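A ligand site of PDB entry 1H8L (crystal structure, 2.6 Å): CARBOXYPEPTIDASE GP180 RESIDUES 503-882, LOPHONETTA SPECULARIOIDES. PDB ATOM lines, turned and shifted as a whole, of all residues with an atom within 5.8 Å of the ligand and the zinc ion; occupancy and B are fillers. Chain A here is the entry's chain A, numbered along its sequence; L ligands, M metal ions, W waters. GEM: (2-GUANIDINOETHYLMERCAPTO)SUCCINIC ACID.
The backbone NH (N) of Asn 141 sits at hydrogen-bond distance from the side-chain carboxylate (OD1) of Asp 139 (2.8 Å).
OE2 of Glu 269 sits close to N of Gly 179 (3.5 Å).
The guanidinium group (NH1) of Arg 132 lies close to the side-chain carboxylate (OE1) of Glu 74 (3.4 Å).
O of Thr 267 sits at hydrogen-bond distance from N of Asn 185, 2.6 Å away.
O of Asn 185 sits close to OE1 of Gln 254 (3.0 Å).
The side-chain carboxylate (OD2) of Asp 139 lies within salt-bridge range of the guanidinium group (NH2) of Arg 142 (3.9 Å).
The side-chain carboxylate of Glu 74 sits close to the backbone NH of Gly 179, 3.0 Å away.
A ring nitrogen (NE2) of His 71 lies close to the guanidinium group (NH2) of Arg 132.
A ring nitrogen (ND1) of His 178 is bound to the zinc ion (2.0 Å).
ND1 of His 71 is bound to the zinc ion, at 2.0 Å.
OE2 of Glu 74 is bound to the zinc ion (2.1 Å).
The zinc ion is bound by O12 of the ligand, at 2.2 Å.
An oxygen (O13) of the ligand binds the zinc ion (2.2 Å).
The side-chain carboxylate (OE1) of Glu 74 is bound to the zinc ion (2.6 Å).
O13 of the ligand sits close to O of Gly 179 (3.5 Å).
O13 of the ligand sits close to OE1 of Glu 269, at 2.9 Å.
Merely in contact with the ligand: Trp 246 and Val 249.
Hydrophobic or aromatic side chains that line the ligand: His 71, His 178, Trp 246, Tyr 247 and Val 249.
Of the 24 residues printed, 14 come within 4 Å of the ligand.
The nearest printed residue that does not touch the ligand is Thr 267 (4.03 Å).
Three residues have an atom within 4 Å of the zinc ion: His 71, Glu 74 and His 178.
The backbone carbonyl oxygen (O) of Gly 243 sits at hydrogen-bond distance from a nitrogen (N4) of the ligand, at 3.2 Å.
The side-chain amide oxygen (OD1) of Asn 185 lies close to a nitrogen (N3) of the ligand (3.4 Å).
O of Tyr 247 lies within hydrogen-bond range of N4 of the ligand (2.5 Å).
An oxygen (O15) of the ligand lies within salt-bridge range of the guanidinium group (NH2) of Arg 142 (2.6 Å).
The side-chain carboxylate of Asp 189 lies within salt-bridge range of a nitrogen (N2) of the ligand (2.5 Å).
NH2 of Arg 132 lies within salt-bridge range of O14 of the ligand.
The side-chain amide nitrogen (ND2) of Asn 141 sits at hydrogen-bond distance from an oxygen (O15) of the ligand (2.9 Å).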
ATOM      1  N   HIS A  71       8.153  17.566  11.628  1.00  0.00           N
ATOM      2  CA  HIS A  71       9.071  17.258  10.558  1.00  0.00           C
ATOM      3  C   HIS A  71      10.206  18.251  10.766  1.00  0.00           C
ATOM      4  O   HIS A  71      10.021  19.456  10.606  1.00  0.00           O
ATOM      5  CB  HIS A  71       8.408  17.473   9.190  1.00  0.00           C
ATOM      6  CG  HIS A  71       7.461  16.378   8.794  1.00  0.00           C
ATOM      7  ND1 HIS A  71       6.365  16.621   8.008  1.00  0.00           N
ATOM      8  CD2 HIS A  71       7.512  15.054   9.098  1.00  0.00           C
ATOM      9  CE1 HIS A  71       5.780  15.456   7.837  1.00  0.00           C
ATOM     10  NE2 HIS A  71       6.431  14.474   8.479  1.00  0.00           N
ATOM     11  N   GLU A  74      10.751  21.578   8.667  1.00  0.00           N
ATOM     12  CA  GLU A  74       9.612  22.485   8.468  1.00  0.00           C
ATOM     13  C   GLU A  74       9.602  23.285   9.768  1.00  0.00           C
ATOM     14  O   GLU A  74       8.917  22.970  10.734  1.00  0.00           O
ATOM     15  CB  GLU A  74       8.341  21.670   8.268  1.00  0.00           C
ATOM     16  CG  GLU A  74       8.464  20.778   7.039  1.00  0.00           C
ATOM     17  CD  GLU A  74       7.310  19.820   6.873  1.00  0.00           C
ATOM     18  OE1 GLU A  74       7.413  18.928   5.998  1.00  0.00           O
ATOM     19  OE2 GLU A  74       6.316  19.943   7.620  1.00  0.00           O
ATOM     20  N   ARG A 132      13.859  15.879   7.989  1.00  0.00           N
ATOM     21  CA  ARG A 132      12.425  15.631   8.065  1.00  0.00           C
ATOM     22  C   ARG A 132      12.067  14.502   9.027  1.00  0.00           C
ATOM     23  O   ARG A 132      11.289  14.709   9.961  1.00  0.00           O
ATOM     24  CB  ARG A 132      11.880  15.312   6.678  1.00  0.00           C
ATOM     25  CG  ARG A 132      10.415  14.904   6.675  1.00  0.00           C
ATOM     26  CD  ARG A 132      10.013  14.434   5.310  1.00  0.00           C
ATOM     27  NE  ARG A 132       8.716  13.749   5.301  1.00  0.00           N
ATOM     28  CZ  ARG A 132       7.542  14.351   5.132  1.00  0.00           C
ATOM     29  NH1 ARG A 132       7.474  15.674   4.957  1.00  0.00           N
ATOM     30  NH2 ARG A 132       6.421  13.630   5.139  1.00  0.00           N
ATOM     31  N   ASP A 139       9.350   8.589   9.480  1.00  0.00           N
ATOM     32  CA  ASP A 139       8.494   9.759   9.369  1.00  0.00           C
ATOM     33  C   ASP A 139       7.492   9.712  10.526  1.00  0.00           C
ATOM     34  O   ASP A 139       6.634   8.824  10.582  1.00  0.00           O
ATOM     35  CB  ASP A 139       7.731   9.737   8.052  1.00  0.00           C
ATOM     36  CG  ASP A 139       7.075  11.062   7.731  1.00  0.00           C
ATOM     37  OD1 ASP A 139       6.515  11.689   8.650  1.00  0.00           O
ATOM     38  OD2 ASP A 139       7.117  11.475   6.543  1.00  0.00           O
ATOM     39  N   ASN A 141       5.029  11.438  10.980  1.00  0.00           N
ATOM     40  CA  ASN A 141       3.665  11.638  10.510  1.00  0.00           C
ATOM     41  C   ASN A 141       3.196  10.484   9.618  1.00  0.00           C
ATOM     42  O   ASN A 141       2.323  10.641   8.774  1.00  0.00           O
ATOM     43  CB  ASN A 141       3.525  12.974   9.785  1.00  0.00           C
ATOM     44  CG  ASN A 141       2.083  13.459   9.709  1.00  0.00           C
ATOM     45  OD1 ASN A 141       1.320  13.343  10.675  1.00  0.00           O
ATOM     46  ND2 ASN A 141       1.707  14.007   8.570  1.00  0.00           N
ATOM     47  N   ARG A 142       3.806   9.320   9.828  1.00  0.00           N
ATOM     48  CA  ARG A 142       3.477   8.079   9.136  1.00  0.00           C
ATOM     49  C   ARG A 142       3.533   7.024  10.230  1.00  0.00           C
ATOM     50  O   ARG A 142       3.226   5.854  10.008  1.00  0.00           O
ATOM     51  CB  ARG A 142       4.529   7.720   8.094  1.00  0.00           C
ATOM     52  CG  ARG A 142       4.624   8.667   6.951  1.00  0.00           C
ATOM     53  CD  ARG A 142       3.380   8.582   6.078  1.00  0.00           C
ATOM     54  NE  ARG A 142       3.485   9.496   4.949  1.00  0.00           N
ATOM     55  CZ  ARG A 142       3.412  10.815   5.058  1.00  0.00           C
ATOM     56  NH1 ARG A 142       3.529  11.578   3.983  1.00  0.00           N
ATOM     57  NH2 ARG A 142       3.185  11.370   6.237  1.00  0.00           N
ATOM     58  N   LEU A 177       1.544  22.072  13.198  1.00  0.00           N
ATOM     59  CA  LEU A 177       2.078  22.879  12.103  1.00  0.00           C
ATOM     60  C   LEU A 177       3.153  22.267  11.222  1.00  0.00           C
ATOM     61  O   LEU A 177       4.080  21.626  11.699  1.00  0.00           O
ATOM     62  CB  LEU A 177       2.574  24.196  12.682  1.00  0.00           C
ATOM     63  CG  LEU A 177       1.673  24.746  13.785  1.00  0.00           C
ATOM     64  CD1 LEU A 177       2.254  26.016  14.361  1.00  0.00           C
ATOM     65  CD2 LEU A 177       0.293  25.017  13.225  1.00  0.00           C
ATOM     66  N   HIS A 178       3.026  22.522   9.918  1.00  0.00           N
ATOM     67  CA  HIS A 178       3.974  22.025   8.921  1.00  0.00           C
ATOM     68  C   HIS A 178       4.389  23.109   7.931  1.00  0.00           C
ATOM     69  O   HIS A 178       3.949  24.261   8.009  1.00  0.00           O
ATOM     70  CB  HIS A 178       3.349  20.884   8.112  1.00  0.00           C
ATOM     71  CG  HIS A 178       3.148  19.630   8.887  1.00  0.00           C
ATOM     72  ND1 HIS A 178       3.897  18.505   8.650  1.00  0.00           N
ATOM     73  CD2 HIS A 178       2.257  19.375   9.889  1.00  0.00           C
ATOM     74  CE1 HIS A 178       3.449  17.594   9.486  1.00  0.00           C
ATOM     75  NE2 HIS A 178       2.461  18.069  10.264  1.00  0.00           N
ATOM     76  N   GLY A 179       5.230  22.714   6.990  1.00  0.00           N
ATOM     77  CA  GLY A 179       5.715  23.600   5.959  1.00  0.00           C
ATOM     78  C   GLY A 179       5.821  22.811   4.666  1.00  0.00           C
ATOM     79  O   GLY A 179       5.971  21.590   4.697  1.00  0.00           O
ATOM     80  N   GLY A 180       5.744  23.496   3.546  1.00  0.00           N
ATOM     81  CA  GLY A 180       5.827  22.808   2.263  1.00  0.00           C
ATOM     82  C   GLY A 180       4.631  23.185   1.419  1.00  0.00           C
ATOM     83  O   GLY A 180       4.496  22.717   0.290  1.00  0.00           O
ATOM     84  N   ASN A 185      -5.189  21.842   6.398  1.00  0.00           N
ATOM     85  CA  ASN A 185      -5.556  20.466   6.064  1.00  0.00           C
ATOM     86  C   ASN A 185      -6.439  19.821   7.151  1.00  0.00           C
ATOM     87  O   ASN A 185      -6.093  19.873   8.336  1.00  0.00           O
ATOM     88  CB  ASN A 185      -4.232  19.704   5.913  1.00  0.00           C
ATOM     89  CG  ASN A 185      -4.394  18.264   5.504  1.00  0.00           C
ATOM     90  OD1 ASN A 185      -4.341  17.948   4.312  1.00  0.00           O
ATOM     91  ND2 ASN A 185      -4.575  17.382   6.469  1.00  0.00           N
ATOM     92  N   PHE A 188     -10.514  13.307   6.740  1.00  0.00           N
ATOM     93  CA  PHE A 188      -9.453  12.323   6.960  1.00  0.00           C
ATOM     94  C   PHE A 188      -8.264  12.516   6.010  1.00  0.00           C
ATOM     95  O   PHE A 188      -8.430  13.053   4.911  1.00  0.00           O
ATOM     96  CB  PHE A 188     -10.004  10.915   6.757  1.00  0.00           C
ATOM     97  CG  PHE A 188     -10.989  10.498   7.796  1.00  0.00           C
ATOM     98  CD1 PHE A 188     -10.663  10.584   9.150  1.00  0.00           C
ATOM     99  CD2 PHE A 188     -12.223   9.999   7.431  1.00  0.00           C
ATOM    100  CE1 PHE A 188     -11.561  10.157  10.121  1.00  0.00           C
ATOM    101  CE2 PHE A 188     -13.132   9.564   8.384  1.00  0.00           C
ATOM    102  CZ  PHE A 188     -12.807   9.650   9.738  1.00  0.00           C
ATOM    103  N   ASP A 189      -7.078  12.063   6.441  1.00  0.00           N
ATOM    104  CA  ASP A 189      -5.858  12.194   5.651  1.00  0.00           C
ATOM    105  C   ASP A 189      -5.658  11.094   4.625  1.00  0.00           C
ATOM    106  O   ASP A 189      -4.806  11.201   3.742  1.00  0.00           O
ATOM    107  CB  ASP A 189      -4.619  12.195   6.549  1.00  0.00           C
ATOM    108  CG  ASP A 189      -4.242  13.579   6.998  1.00  0.00           C
ATOM    109  OD1 ASP A 189      -4.457  14.533   6.232  1.00  0.00           O
ATOM    110  OD2 ASP A 189      -3.704  13.696   8.117  1.00  0.00           O
ATOM    111  N   ASP A 190      -6.438  10.027   4.745  1.00  0.00           N
ATOM    112  CA  ASP A 190      -6.312   8.917   3.816  1.00  0.00           C
ATOM    113  C   ASP A 190      -7.652   8.222   3.675  1.00  0.00           C
ATOM    114  O   ASP A 190      -8.614   8.551   4.360  1.00  0.00           O
ATOM    115  CB  ASP A 190      -5.230   7.955   4.303  1.00  0.00           C
ATOM    116  CG  ASP A 190      -5.635   7.184   5.555  1.00  0.00           C
ATOM    117  OD1 ASP A 190      -6.406   7.704   6.389  1.00  0.00           O
ATOM    118  OD2 ASP A 190      -5.163   6.042   5.695  1.00  0.00           O
ATOM    119  N   ASN A 242      -9.228  18.939   2.305  1.00  0.00           N
ATOM    120  CA  ASN A 242      -9.396  17.664   2.967  1.00  0.00           C
ATOM    121  C   ASN A 242      -8.044  16.995   2.723  1.00  0.00           C
ATOM    122  O   ASN A 242      -7.497  17.097   1.629  1.00  0.00           O
ATOM    123  CB  ASN A 242     -10.548  16.885   2.328  1.00  0.00           C
ATOM    124  CG  ASN A 242     -10.521  15.395   2.654  1.00  0.00           C
ATOM    125  OD1 ASN A 242     -10.153  14.584   1.816  1.00  0.00           O
ATOM    126  ND2 ASN A 242     -10.922  15.044   3.874  1.00  0.00           N
ATOM    127  N   GLY A 243      -7.502  16.336   3.744  1.00  0.00           N
ATOM    128  CA  GLY A 243      -6.211  15.702   3.581  1.00  0.00           C
ATOM    129  C   GLY A 243      -6.127  14.774   2.382  1.00  0.00           C
ATOM    130  O   GLY A 243      -5.385  15.013   1.430  1.00  0.00           O
ATOM    131  N   ALA A 244      -6.905  13.694   2.444  1.00  0.00           N
ATOM    132  CA  ALA A 244      -6.937  12.676   1.399  1.00  0.00           C
ATOM    133  C   ALA A 244      -7.081  13.227  -0.010  1.00  0.00           C
ATOM    134  O   ALA A 244      -6.444  12.721  -0.935  1.00  0.00           O
ATOM    135  CB  ALA A 244      -8.051  11.686   1.670  1.00  0.00           C
ATOM    136  N   TRP A 246      -6.074  16.021  -1.213  1.00  0.00           N
ATOM    137  CA  TRP A 246      -4.816  16.609  -1.647  1.00  0.00           C
ATOM    138  C   TRP A 246      -3.965  15.396  -2.063  1.00  0.00           C
ATOM    139  O   TRP A 246      -3.454  15.338  -3.193  1.00  0.00           O
ATOM    140  CB  TRP A 246      -4.198  17.371  -0.482  1.00  0.00           C
ATOM    141  CG  TRP A 246      -2.954  18.064  -0.829  1.00  0.00           C
ATOM    142  CD1 TRP A 246      -2.410  18.199  -2.078  1.00  0.00           C
ATOM    143  CD2 TRP A 246      -2.048  18.712   0.077  1.00  0.00           C
ATOM    144  NE1 TRP A 246      -1.223  18.894  -2.009  1.00  0.00           N
ATOM    145  CE2 TRP A 246      -0.974  19.215  -0.689  1.00  0.00           C
ATOM    146  CE3 TRP A 246      -2.043  18.901   1.471  1.00  0.00           C
ATOM    147  CZ2 TRP A 246       0.095  19.911  -0.118  1.00  0.00           C
ATOM    148  CZ3 TRP A 246      -0.980  19.592   2.047  1.00  0.00           C
ATOM    149  CH2 TRP A 246       0.074  20.086   1.253  1.00  0.00           C
ATOM    150  N   TYR A 247      -3.821  14.444  -1.156  1.00  0.00           N
ATOM    151  CA  TYR A 247      -3.113  13.195  -1.420  1.00  0.00           C
ATOM    152  C   TYR A 247      -3.161  12.286  -0.199  1.00  0.00           C
ATOM    153  O   TYR A 247      -3.212  12.769   0.935  1.00  0.00           O
ATOM    154  CB  TYR A 247      -1.681  13.447  -1.916  1.00  0.00           C
ATOM    155  CG  TYR A 247      -0.717  14.057  -0.934  1.00  0.00           C
ATOM    156  CD1 TYR A 247       0.014  13.256  -0.051  1.00  0.00           C
ATOM    157  CD2 TYR A 247      -0.477  15.439  -0.934  1.00  0.00           C
ATOM    158  CE1 TYR A 247       0.956  13.816   0.804  1.00  0.00           C
ATOM    159  CE2 TYR A 247       0.465  15.999  -0.080  1.00  0.00           C
ATOM    160  CZ  TYR A 247       1.177  15.178   0.785  1.00  0.00           C
ATOM    161  OH  TYR A 247       2.135  15.728   1.616  1.00  0.00           O
ATOM    162  N   ASN A 248      -3.192  10.988  -0.427  1.00  0.00           N
ATOM    163  CA  ASN A 248      -3.291  10.008   0.638  1.00  0.00           C
ATOM    164  C   ASN A 248      -2.074   9.986   1.576  1.00  0.00           C
ATOM    165  O   ASN A 248      -0.928   9.905   1.128  1.00  0.00           O
ATOM    166  CB  ASN A 248      -3.518   8.622   0.013  1.00  0.00           C
ATOM    167  CG  ASN A 248      -4.001   7.599   1.018  1.00  0.00           C
ATOM    168  OD1 ASN A 248      -5.167   7.604   1.417  1.00  0.00           O
ATOM    169  ND2 ASN A 248      -3.106   6.712   1.427  1.00  0.00           N
ATOM    170  N   VAL A 249      -2.355  10.062   2.869  1.00  0.00           N
ATOM    171  CA  VAL A 249      -1.320  10.026   3.907  1.00  0.00           C
ATOM    172  C   VAL A 249      -1.760   9.125   5.052  1.00  0.00           C
ATOM    173  O   VAL A 249      -2.666   9.479   5.798  1.00  0.00           O
ATOM    174  CB  VAL A 249      -1.039  11.420   4.511  1.00  0.00           C
ATOM    175  CG1 VAL A 249      -0.157  11.283   5.738  1.00  0.00           C
ATOM    176  CG2 VAL A 249      -0.356  12.316   3.491  1.00  0.00           C
ATOM    177  N   GLN A 254      -2.739  13.638  12.905  1.00  0.00           N
ATOM    178  CA  GLN A 254      -4.015  14.345  12.816  1.00  0.00           C
ATOM    179  C   GLN A 254      -5.263  13.466  12.976  1.00  0.00           C
ATOM    180  O   GLN A 254      -6.153  13.778  13.770  1.00  0.00           O
ATOM    181  CB  GLN A 254      -4.085  15.079  11.482  1.00  0.00           C
ATOM    182  CG  GLN A 254      -5.450  15.626  11.176  1.00  0.00           C
ATOM    183  CD  GLN A 254      -5.557  16.142   9.776  1.00  0.00           C
ATOM    184  OE1 GLN A 254      -5.105  17.243   9.470  1.00  0.00           O
ATOM    185  NE2 GLN A 254      -6.142  15.349   8.911  1.00  0.00           N
ATOM    186  N   THR A 267      -4.316  20.117  10.471  1.00  0.00           N
ATOM    187  CA  THR A 267      -2.904  20.269  10.100  1.00  0.00           C
ATOM    188  C   THR A 267      -2.711  21.563   9.317  1.00  0.00           C
ATOM    189  O   THR A 267      -3.340  21.767   8.284  1.00  0.00           O
ATOM    190  CB  THR A 267      -2.432  19.107   9.216  1.00  0.00           C
ATOM    191  OG1 THR A 267      -2.703  17.861   9.863  1.00  0.00           O
ATOM    192  CG2 THR A 267      -0.953  19.210   8.972  1.00  0.00           C
ATOM    193  N   GLU A 269      -0.354  24.179   7.108  1.00  0.00           N
ATOM    194  CA  GLU A 269       0.831  24.363   6.277  1.00  0.00           C
ATOM    195  C   GLU A 269       1.064  25.866   6.222  1.00  0.00           C
ATOM    196  O   GLU A 269       0.282  26.599   5.623  1.00  0.00           O
ATOM    197  CB  GLU A 269       0.578  23.794   4.884  1.00  0.00           C
ATOM    198  CG  GLU A 269       0.332  22.289   4.875  1.00  0.00           C
ATOM    199  CD  GLU A 269       1.616  21.475   4.854  1.00  0.00           C
ATOM    200  OE1 GLU A 269       1.548  20.230   4.989  1.00  0.00           O
ATOM    201  OE2 GLU A 269       2.694  22.084   4.697  1.00  0.00           O
HETATM  202  C8  GEM L   1       2.064  15.999   4.787  1.00  0.00           C
HETATM  203  S7  GEM L   1       0.945  16.225   6.192  1.00  0.00           S
HETATM  204  C6  GEM L   1      -0.287  17.318   5.482  1.00  0.00           C
HETATM  205  C5  GEM L   1      -1.544  16.542   5.130  1.00  0.00           C
HETATM  206  N3  GEM L   1      -1.528  16.070   3.759  1.00  0.00           N
HETATM  207  C1  GEM L   1      -2.269  15.063   3.299  1.00  0.00           C
HETATM  208  N4  GEM L   1      -2.211  14.726   2.029  1.00  0.00           N
HETATM  209  N2  GEM L   1      -3.086  14.405   4.117  1.00  0.00           N
HETATM  210  C9  GEM L   1       3.075  14.879   5.077  1.00  0.00           C
HETATM  211  O14 GEM L   1       4.185  14.976   4.556  1.00  0.00           O
HETATM  212  O15 GEM L   1       2.777  13.951   5.838  1.00  0.00           O
HETATM  213  C10 GEM L   1       2.801  17.277   4.356  1.00  0.00           C
HETATM  214  C11 GEM L   1       3.913  17.671   5.295  1.00  0.00           C
HETATM  215  O12 GEM L   1       4.793  16.843   5.624  1.00  0.00           O
HETATM  216  O13 GEM L   1       3.991  18.860   5.598  1.00  0.00           O
HETATM  217 ZN    ZN M   1       5.307  18.163   7.280  1.00  0.00          ZN
HETATM  218  O   HOH W   1       6.152  18.651   3.166  1.00  0.00           O
